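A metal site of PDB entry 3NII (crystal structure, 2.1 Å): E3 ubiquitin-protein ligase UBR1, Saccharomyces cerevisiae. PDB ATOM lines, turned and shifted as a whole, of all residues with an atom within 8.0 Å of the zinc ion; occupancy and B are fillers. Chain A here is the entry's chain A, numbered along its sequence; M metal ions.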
ATOM      1  N   ARG A  23      12.589  -2.862 -26.307  1.00  0.00           N
ATOM      2  CA  ARG A  23      13.722  -2.041 -25.898  1.00  0.00           C
ATOM      3  C   ARG A  23      13.322  -1.157 -24.719  1.00  0.00           C
ATOM      4  O   ARG A  23      12.163  -0.743 -24.619  1.00  0.00           O
ATOM      5  CB  ARG A  23      14.175  -1.147 -27.065  1.00  0.00           C
ATOM      6  CG  ARG A  23      15.330  -1.713 -27.868  1.00  0.00           C
ATOM      7  CD  ARG A  23      15.126  -1.574 -29.375  1.00  0.00           C
ATOM      8  NE  ARG A  23      14.831  -0.212 -29.826  1.00  0.00           N
ATOM      9  CZ  ARG A  23      14.879   0.180 -31.103  1.00  0.00           C
ATOM     10  NH1 ARG A  23      15.224  -0.668 -32.059  1.00  0.00           N
ATOM     11  NH2 ARG A  23      14.585   1.440 -31.414  1.00  0.00           N
ATOM     12  N   CYS A  24      14.272  -0.863 -23.826  1.00  0.00           N
ATOM     13  CA  CYS A  24      14.012   0.023 -22.692  1.00  0.00           C
ATOM     14  C   CYS A  24      15.096   1.085 -22.629  1.00  0.00           C
ATOM     15  O   CYS A  24      16.284   0.761 -22.592  1.00  0.00           O
ATOM     16  CB  CYS A  24      13.947  -0.763 -21.380  1.00  0.00           C
ATOM     17  SG  CYS A  24      13.606   0.267 -19.912  1.00  0.00           S
ATOM     18  N   HIS A  25      14.674   2.350 -22.628  1.00  0.00           N
ATOM     19  CA  HIS A  25      15.598   3.470 -22.623  1.00  0.00           C
ATOM     20  C   HIS A  25      16.583   3.419 -21.446  1.00  0.00           C
ATOM     21  O   HIS A  25      17.789   3.562 -21.646  1.00  0.00           O
ATOM     22  CB  HIS A  25      14.852   4.804 -22.623  1.00  0.00           C
ATOM     23  CG  HIS A  25      15.749   6.000 -22.709  1.00  0.00           C
ATOM     24  ND1 HIS A  25      16.461   6.322 -23.850  1.00  0.00           N
ATOM     25  CD2 HIS A  25      16.077   6.937 -21.783  1.00  0.00           C
ATOM     26  CE1 HIS A  25      17.177   7.411 -23.625  1.00  0.00           C
ATOM     27  NE2 HIS A  25      16.960   7.803 -22.373  1.00  0.00           N
ATOM     28  N   GLU A  26      16.071   3.210 -20.234  1.00  0.00           N
ATOM     29  CA  GLU A  26      16.906   3.201 -19.032  1.00  0.00           C
ATOM     30  C   GLU A  26      17.637   1.893 -18.779  1.00  0.00           C
ATOM     31  O   GLU A  26      18.779   1.915 -18.307  1.00  0.00           O
ATOM     32  CB  GLU A  26      16.140   3.643 -17.775  1.00  0.00           C
ATOM     33  CG  GLU A  26      14.636   3.382 -17.796  1.00  0.00           C
ATOM     34  CD  GLU A  26      13.879   4.404 -18.630  1.00  0.00           C
ATOM     35  OE1 GLU A  26      14.173   5.616 -18.537  1.00  0.00           O
ATOM     36  OE2 GLU A  26      12.996   3.992 -19.401  1.00  0.00           O
ATOM     37  N   CYS A  27      17.002   0.762 -19.086  1.00  0.00           N
ATOM     38  CA  CYS A  27      17.597  -0.542 -18.809  1.00  0.00           C
ATOM     39  C   CYS A  27      18.644  -0.931 -19.855  1.00  0.00           C
ATOM     40  O   CYS A  27      19.656  -1.546 -19.514  1.00  0.00           O
ATOM     41  CB  CYS A  27      16.524  -1.629 -18.697  1.00  0.00           C
ATOM     42  SG  CYS A  27      15.381  -1.360 -17.315  1.00  0.00           S
ATOM     43  N   GLY A  28      18.401  -0.561 -21.112  1.00  0.00           N
ATOM     44  CA  GLY A  28      19.314  -0.869 -22.200  1.00  0.00           C
ATOM     45  C   GLY A  28      20.634  -0.115 -22.158  1.00  0.00           C
ATOM     46  O   GLY A  28      20.645   1.114 -22.132  1.00  0.00           O
ATOM     47  N   LEU A  35      14.911  -7.346 -25.974  1.00  0.00           N
ATOM     48  CA  LEU A  35      14.325  -8.513 -25.337  1.00  0.00           C
ATOM     49  C   LEU A  35      13.217  -9.075 -26.213  1.00  0.00           C
ATOM     50  O   LEU A  35      12.514  -8.318 -26.880  1.00  0.00           O
ATOM     51  CB  LEU A  35      13.749  -8.156 -23.965  1.00  0.00           C
ATOM     52  CG  LEU A  35      14.725  -7.656 -22.898  1.00  0.00           C
ATOM     53  CD1 LEU A  35      14.001  -6.858 -21.816  1.00  0.00           C
ATOM     54  CD2 LEU A  35      15.493  -8.827 -22.282  1.00  0.00           C
ATOM     55  N   PHE A  40      10.882 -10.493 -21.932  1.00  0.00           N
ATOM     56  CA  PHE A  40      10.463  -9.185 -21.401  1.00  0.00           C
ATOM     57  C   PHE A  40       9.466  -9.329 -20.246  1.00  0.00           C
ATOM     58  O   PHE A  40       8.378  -9.905 -20.410  1.00  0.00           O
ATOM     59  CB  PHE A  40       9.884  -8.304 -22.500  1.00  0.00           C
ATOM     60  CG  PHE A  40       9.415  -6.942 -22.018  1.00  0.00           C
ATOM     61  CD1 PHE A  40      10.321  -5.898 -21.866  1.00  0.00           C
ATOM     62  CD2 PHE A  40       8.067  -6.713 -21.737  1.00  0.00           C
ATOM     63  CE1 PHE A  40       9.889  -4.634 -21.430  1.00  0.00           C
ATOM     64  CE2 PHE A  40       7.629  -5.461 -21.295  1.00  0.00           C
ATOM     65  CZ  PHE A  40       8.545  -4.427 -21.139  1.00  0.00           C
ATOM     66  N   ASN A  41       9.850  -8.794 -19.091  1.00  0.00           N
ATOM     67  CA  ASN A  41       8.984  -8.785 -17.921  1.00  0.00           C
ATOM     68  C   ASN A  41       8.549  -7.361 -17.605  1.00  0.00           C
ATOM     69  O   ASN A  41       9.364  -6.540 -17.204  1.00  0.00           O
ATOM     70  CB  ASN A  41       9.703  -9.413 -16.724  1.00  0.00           C
ATOM     71  CG  ASN A  41       8.754  -9.879 -15.629  1.00  0.00           C
ATOM     72  OD1 ASN A  41       9.079 -10.766 -14.851  1.00  0.00           O
ATOM     73  ND2 ASN A  41       7.573  -9.275 -15.562  1.00  0.00           N
ATOM     74  N   PRO A  42       7.242  -7.045 -17.797  1.00  0.00           N
ATOM     75  CA  PRO A  42       6.719  -5.704 -17.502  1.00  0.00           C
ATOM     76  C   PRO A  42       7.023  -5.249 -16.079  1.00  0.00           C
ATOM     77  O   PRO A  42       7.150  -4.047 -15.832  1.00  0.00           O
ATOM     78  CB  PRO A  42       5.209  -5.853 -17.718  1.00  0.00           C
ATOM     79  CG  PRO A  42       4.947  -7.322 -17.741  1.00  0.00           C
ATOM     80  CD  PRO A  42       6.179  -7.936 -18.308  1.00  0.00           C
ATOM     81  N   LYS A  43       7.147  -6.201 -15.154  1.00  0.00           N
ATOM     82  CA  LYS A  43       7.461  -5.918 -13.743  1.00  0.00           C
ATOM     83  C   LYS A  43       8.834  -5.271 -13.546  1.00  0.00           C
ATOM     84  O   LYS A  43       9.079  -4.627 -12.522  1.00  0.00           O
ATOM     85  CB  LYS A  43       7.360  -7.211 -12.909  1.00  0.00           C
ATOM     86  CG  LYS A  43       5.948  -7.734 -12.745  1.00  0.00           C
ATOM     87  CD  LYS A  43       5.893  -8.978 -11.856  1.00  0.00           C
ATOM     88  CE  LYS A  43       6.107 -10.257 -12.641  1.00  0.00           C
ATOM     89  NZ  LYS A  43       5.876 -11.468 -11.805  1.00  0.00           N
ATOM     90  N   ASP A  44       9.711  -5.463 -14.528  1.00  0.00           N
ATOM     91  CA  ASP A  44      11.048  -4.895 -14.524  1.00  0.00           C
ATOM     92  C   ASP A  44      11.066  -3.428 -14.975  1.00  0.00           C
ATOM     93  O   ASP A  44      12.040  -2.713 -14.735  1.00  0.00           O
ATOM     94  CB  ASP A  44      11.992  -5.689 -15.448  1.00  0.00           C
ATOM     95  CG  ASP A  44      12.415  -7.034 -14.871  1.00  0.00           C
ATOM     96  OD1 ASP A  44      12.614  -7.137 -13.638  1.00  0.00           O
ATOM     97  OD2 ASP A  44      12.602  -7.974 -15.667  1.00  0.00           O
ATOM     98  N   HIS A  45       9.991  -3.002 -15.649  1.00  0.00           N
ATOM     99  CA  HIS A  45       9.987  -1.727 -16.388  1.00  0.00           C
ATOM    100  C   HIS A  45       8.765  -0.836 -16.146  1.00  0.00           C
ATOM    101  O   HIS A  45       8.319  -0.120 -17.045  1.00  0.00           O
ATOM    102  CB  HIS A  45      10.148  -1.994 -17.885  1.00  0.00           C
ATOM    103  CG  HIS A  45      11.223  -2.984 -18.217  1.00  0.00           C
ATOM    104  ND1 HIS A  45      12.565  -2.648 -18.236  1.00  0.00           N
ATOM    105  CD2 HIS A  45      11.164  -4.299 -18.515  1.00  0.00           C
ATOM    106  CE1 HIS A  45      13.281  -3.716 -18.543  1.00  0.00           C
ATOM    107  NE2 HIS A  45      12.454  -4.729 -18.727  1.00  0.00           N
ATOM    108  N   VAL A  46       8.241  -0.853 -14.917  1.00  0.00           N
ATOM    109  CA  VAL A  46       7.102  -0.008 -14.541  1.00  0.00           C
ATOM    110  C   VAL A  46       7.458   1.467 -14.709  1.00  0.00           C
ATOM    111  O   VAL A  46       8.400   1.962 -14.088  1.00  0.00           O
ATOM    112  CB  VAL A  46       6.608  -0.293 -13.099  1.00  0.00           C
ATOM    113  CG1 VAL A  46       5.427   0.620 -12.734  1.00  0.00           C
ATOM    114  CG2 VAL A  46       6.229  -1.760 -12.934  1.00  0.00           C
ATOM    115  N   ASN A  47       6.702   2.155 -15.578  1.00  0.00           N
ATOM    116  CA  ASN A  47       6.905   3.572 -15.893  1.00  0.00           C
ATOM    117  C   ASN A  47       8.260   3.883 -16.570  1.00  0.00           C
ATOM    118  O   ASN A  47       8.668   5.036 -16.646  1.00  0.00           O
ATOM    119  CB  ASN A  47       6.665   4.464 -14.672  1.00  0.00           C
ATOM    120  CG  ASN A  47       5.184   4.530 -14.263  1.00  0.00           C
ATOM    121  OD1 ASN A  47       4.291   4.379 -15.099  1.00  0.00           O
ATOM    122  ND2 ASN A  47       4.941   4.766 -12.981  1.00  0.00           N
ATOM    123  N   HIS A  48       8.938   2.843 -17.034  1.00  0.00           N
ATOM    124  CA  HIS A  48      10.114   2.996 -17.889  1.00  0.00           C
ATOM    125  C   HIS A  48       9.664   3.374 -19.302  1.00  0.00           C
ATOM    126  O   HIS A  48       8.490   3.219 -19.658  1.00  0.00           O
ATOM    127  CB  HIS A  48      10.945   1.702 -17.912  1.00  0.00           C
ATOM    128  CG  HIS A  48      11.732   1.465 -16.654  1.00  0.00           C
ATOM    129  ND1 HIS A  48      12.794   0.587 -16.594  1.00  0.00           N
ATOM    130  CD2 HIS A  48      11.618   2.002 -15.415  1.00  0.00           C
ATOM    131  CE1 HIS A  48      13.284   0.586 -15.367  1.00  0.00           C
ATOM    132  NE2 HIS A  48      12.595   1.444 -14.639  1.00  0.00           N
ATOM    133  N   HIS A  49      10.588   3.897 -20.100  1.00  0.00           N
ATOM    134  CA  HIS A  49      10.278   4.278 -21.463  1.00  0.00           C
ATOM    135  C   HIS A  49      10.529   3.090 -22.401  1.00  0.00           C
ATOM    136  O   HIS A  49      11.585   2.975 -23.019  1.00  0.00           O
ATOM    137  CB  HIS A  49      11.071   5.506 -21.879  1.00  0.00           C
ATOM    138  CG  HIS A  49      10.795   6.711 -21.037  1.00  0.00           C
ATOM    139  ND1 HIS A  49      11.549   7.028 -19.922  1.00  0.00           N
ATOM    140  CD2 HIS A  49       9.833   7.664 -21.122  1.00  0.00           C
ATOM    141  CE1 HIS A  49      11.069   8.124 -19.367  1.00  0.00           C
ATOM    142  NE2 HIS A  49      10.038   8.535 -20.079  1.00  0.00           N
ATOM    143  N   VAL A  50       9.536   2.198 -22.463  1.00  0.00           N
ATOM    144  CA  VAL A  50       9.650   0.962 -23.236  1.00  0.00           C
ATOM    145  C   VAL A  50       9.173   1.163 -24.665  1.00  0.00           C
ATOM    146  O   VAL A  50       8.082   1.693 -24.912  1.00  0.00           O
ATOM    147  CB  VAL A  50       8.917  -0.217 -22.563  1.00  0.00           C
ATOM    148  CG1 VAL A  50       9.061  -1.520 -23.388  1.00  0.00           C
ATOM    149  CG2 VAL A  50       9.447  -0.437 -21.150  1.00  0.00           C
ATOM    150  N   TRP A  71      22.670  -4.764 -20.101  1.00  0.00           N
ATOM    151  CA  TRP A  71      21.668  -4.144 -19.232  1.00  0.00           C
ATOM    152  C   TRP A  71      22.247  -3.399 -18.030  1.00  0.00           C
ATOM    153  O   TRP A  71      23.259  -3.802 -17.467  1.00  0.00           O
ATOM    154  CB  TRP A  71      20.643  -5.201 -18.786  1.00  0.00           C
ATOM    155  CG  TRP A  71      20.068  -5.954 -19.947  1.00  0.00           C
ATOM    156  CD1 TRP A  71      20.370  -7.230 -20.335  1.00  0.00           C
ATOM    157  CD2 TRP A  71      19.137  -5.450 -20.920  1.00  0.00           C
ATOM    158  NE1 TRP A  71      19.673  -7.553 -21.472  1.00  0.00           N
ATOM    159  CE2 TRP A  71      18.905  -6.483 -21.854  1.00  0.00           C
ATOM    160  CE3 TRP A  71      18.471  -4.224 -21.080  1.00  0.00           C
ATOM    161  CZ2 TRP A  71      18.039  -6.338 -22.940  1.00  0.00           C
ATOM    162  CZ3 TRP A  71      17.605  -4.079 -22.166  1.00  0.00           C
ATOM    163  CH2 TRP A  71      17.392  -5.124 -23.075  1.00  0.00           C
ATOM    164  N   SER A  73      20.289  -2.696 -15.286  1.00  0.00           N
ATOM    165  CA  SER A  73      19.630  -3.253 -14.118  1.00  0.00           C
ATOM    166  C   SER A  73      19.521  -4.771 -14.232  1.00  0.00           C
ATOM    167  O   SER A  73      19.484  -5.296 -15.351  1.00  0.00           O
ATOM    168  CB  SER A  73      18.239  -2.639 -13.925  1.00  0.00           C
ATOM    169  OG  SER A  73      18.327  -1.280 -13.520  1.00  0.00           O
ATOM    170  N   LEU A  75      17.746  -8.040 -14.651  1.00  0.00           N
ATOM    171  CA  LEU A  75      16.455  -8.421 -15.211  1.00  0.00           C
ATOM    172  C   LEU A  75      15.943  -9.732 -14.618  1.00  0.00           C
ATOM    173  O   LEU A  75      16.722 -10.530 -14.090  1.00  0.00           O
ATOM    174  CB  LEU A  75      16.543  -8.506 -16.744  1.00  0.00           C
ATOM    175  CG  LEU A  75      16.117  -7.291 -17.585  1.00  0.00           C
ATOM    176  CD1 LEU A  75      16.454  -5.939 -16.949  1.00  0.00           C
ATOM    177  CD2 LEU A  75      16.689  -7.372 -18.997  1.00  0.00           C
HETATM  178 ZN    ZN M   1      13.463  -0.867 -18.101  1.00  0.00          ZN
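Four residues have an atom within 4 Å of the zinc ion: Cys 24, Cys 27, His 45 and His 48. Along chain A the residues within 4 Å of the zinc ion span positions 24 to 48.
ND1 of His 45 binds the zinc ion (2.0 Å). The zinc ion is bound by the side-chain sulfur (SG) of Cys 27 (2.1 Å). SG of Cys 24 is bound to the zinc ion, at 2.1 Å. A ring nitrogen (ND1) of His 48 binds the zinc ion (2.2 Å). The zinc ion has four donor atoms within binding distance.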
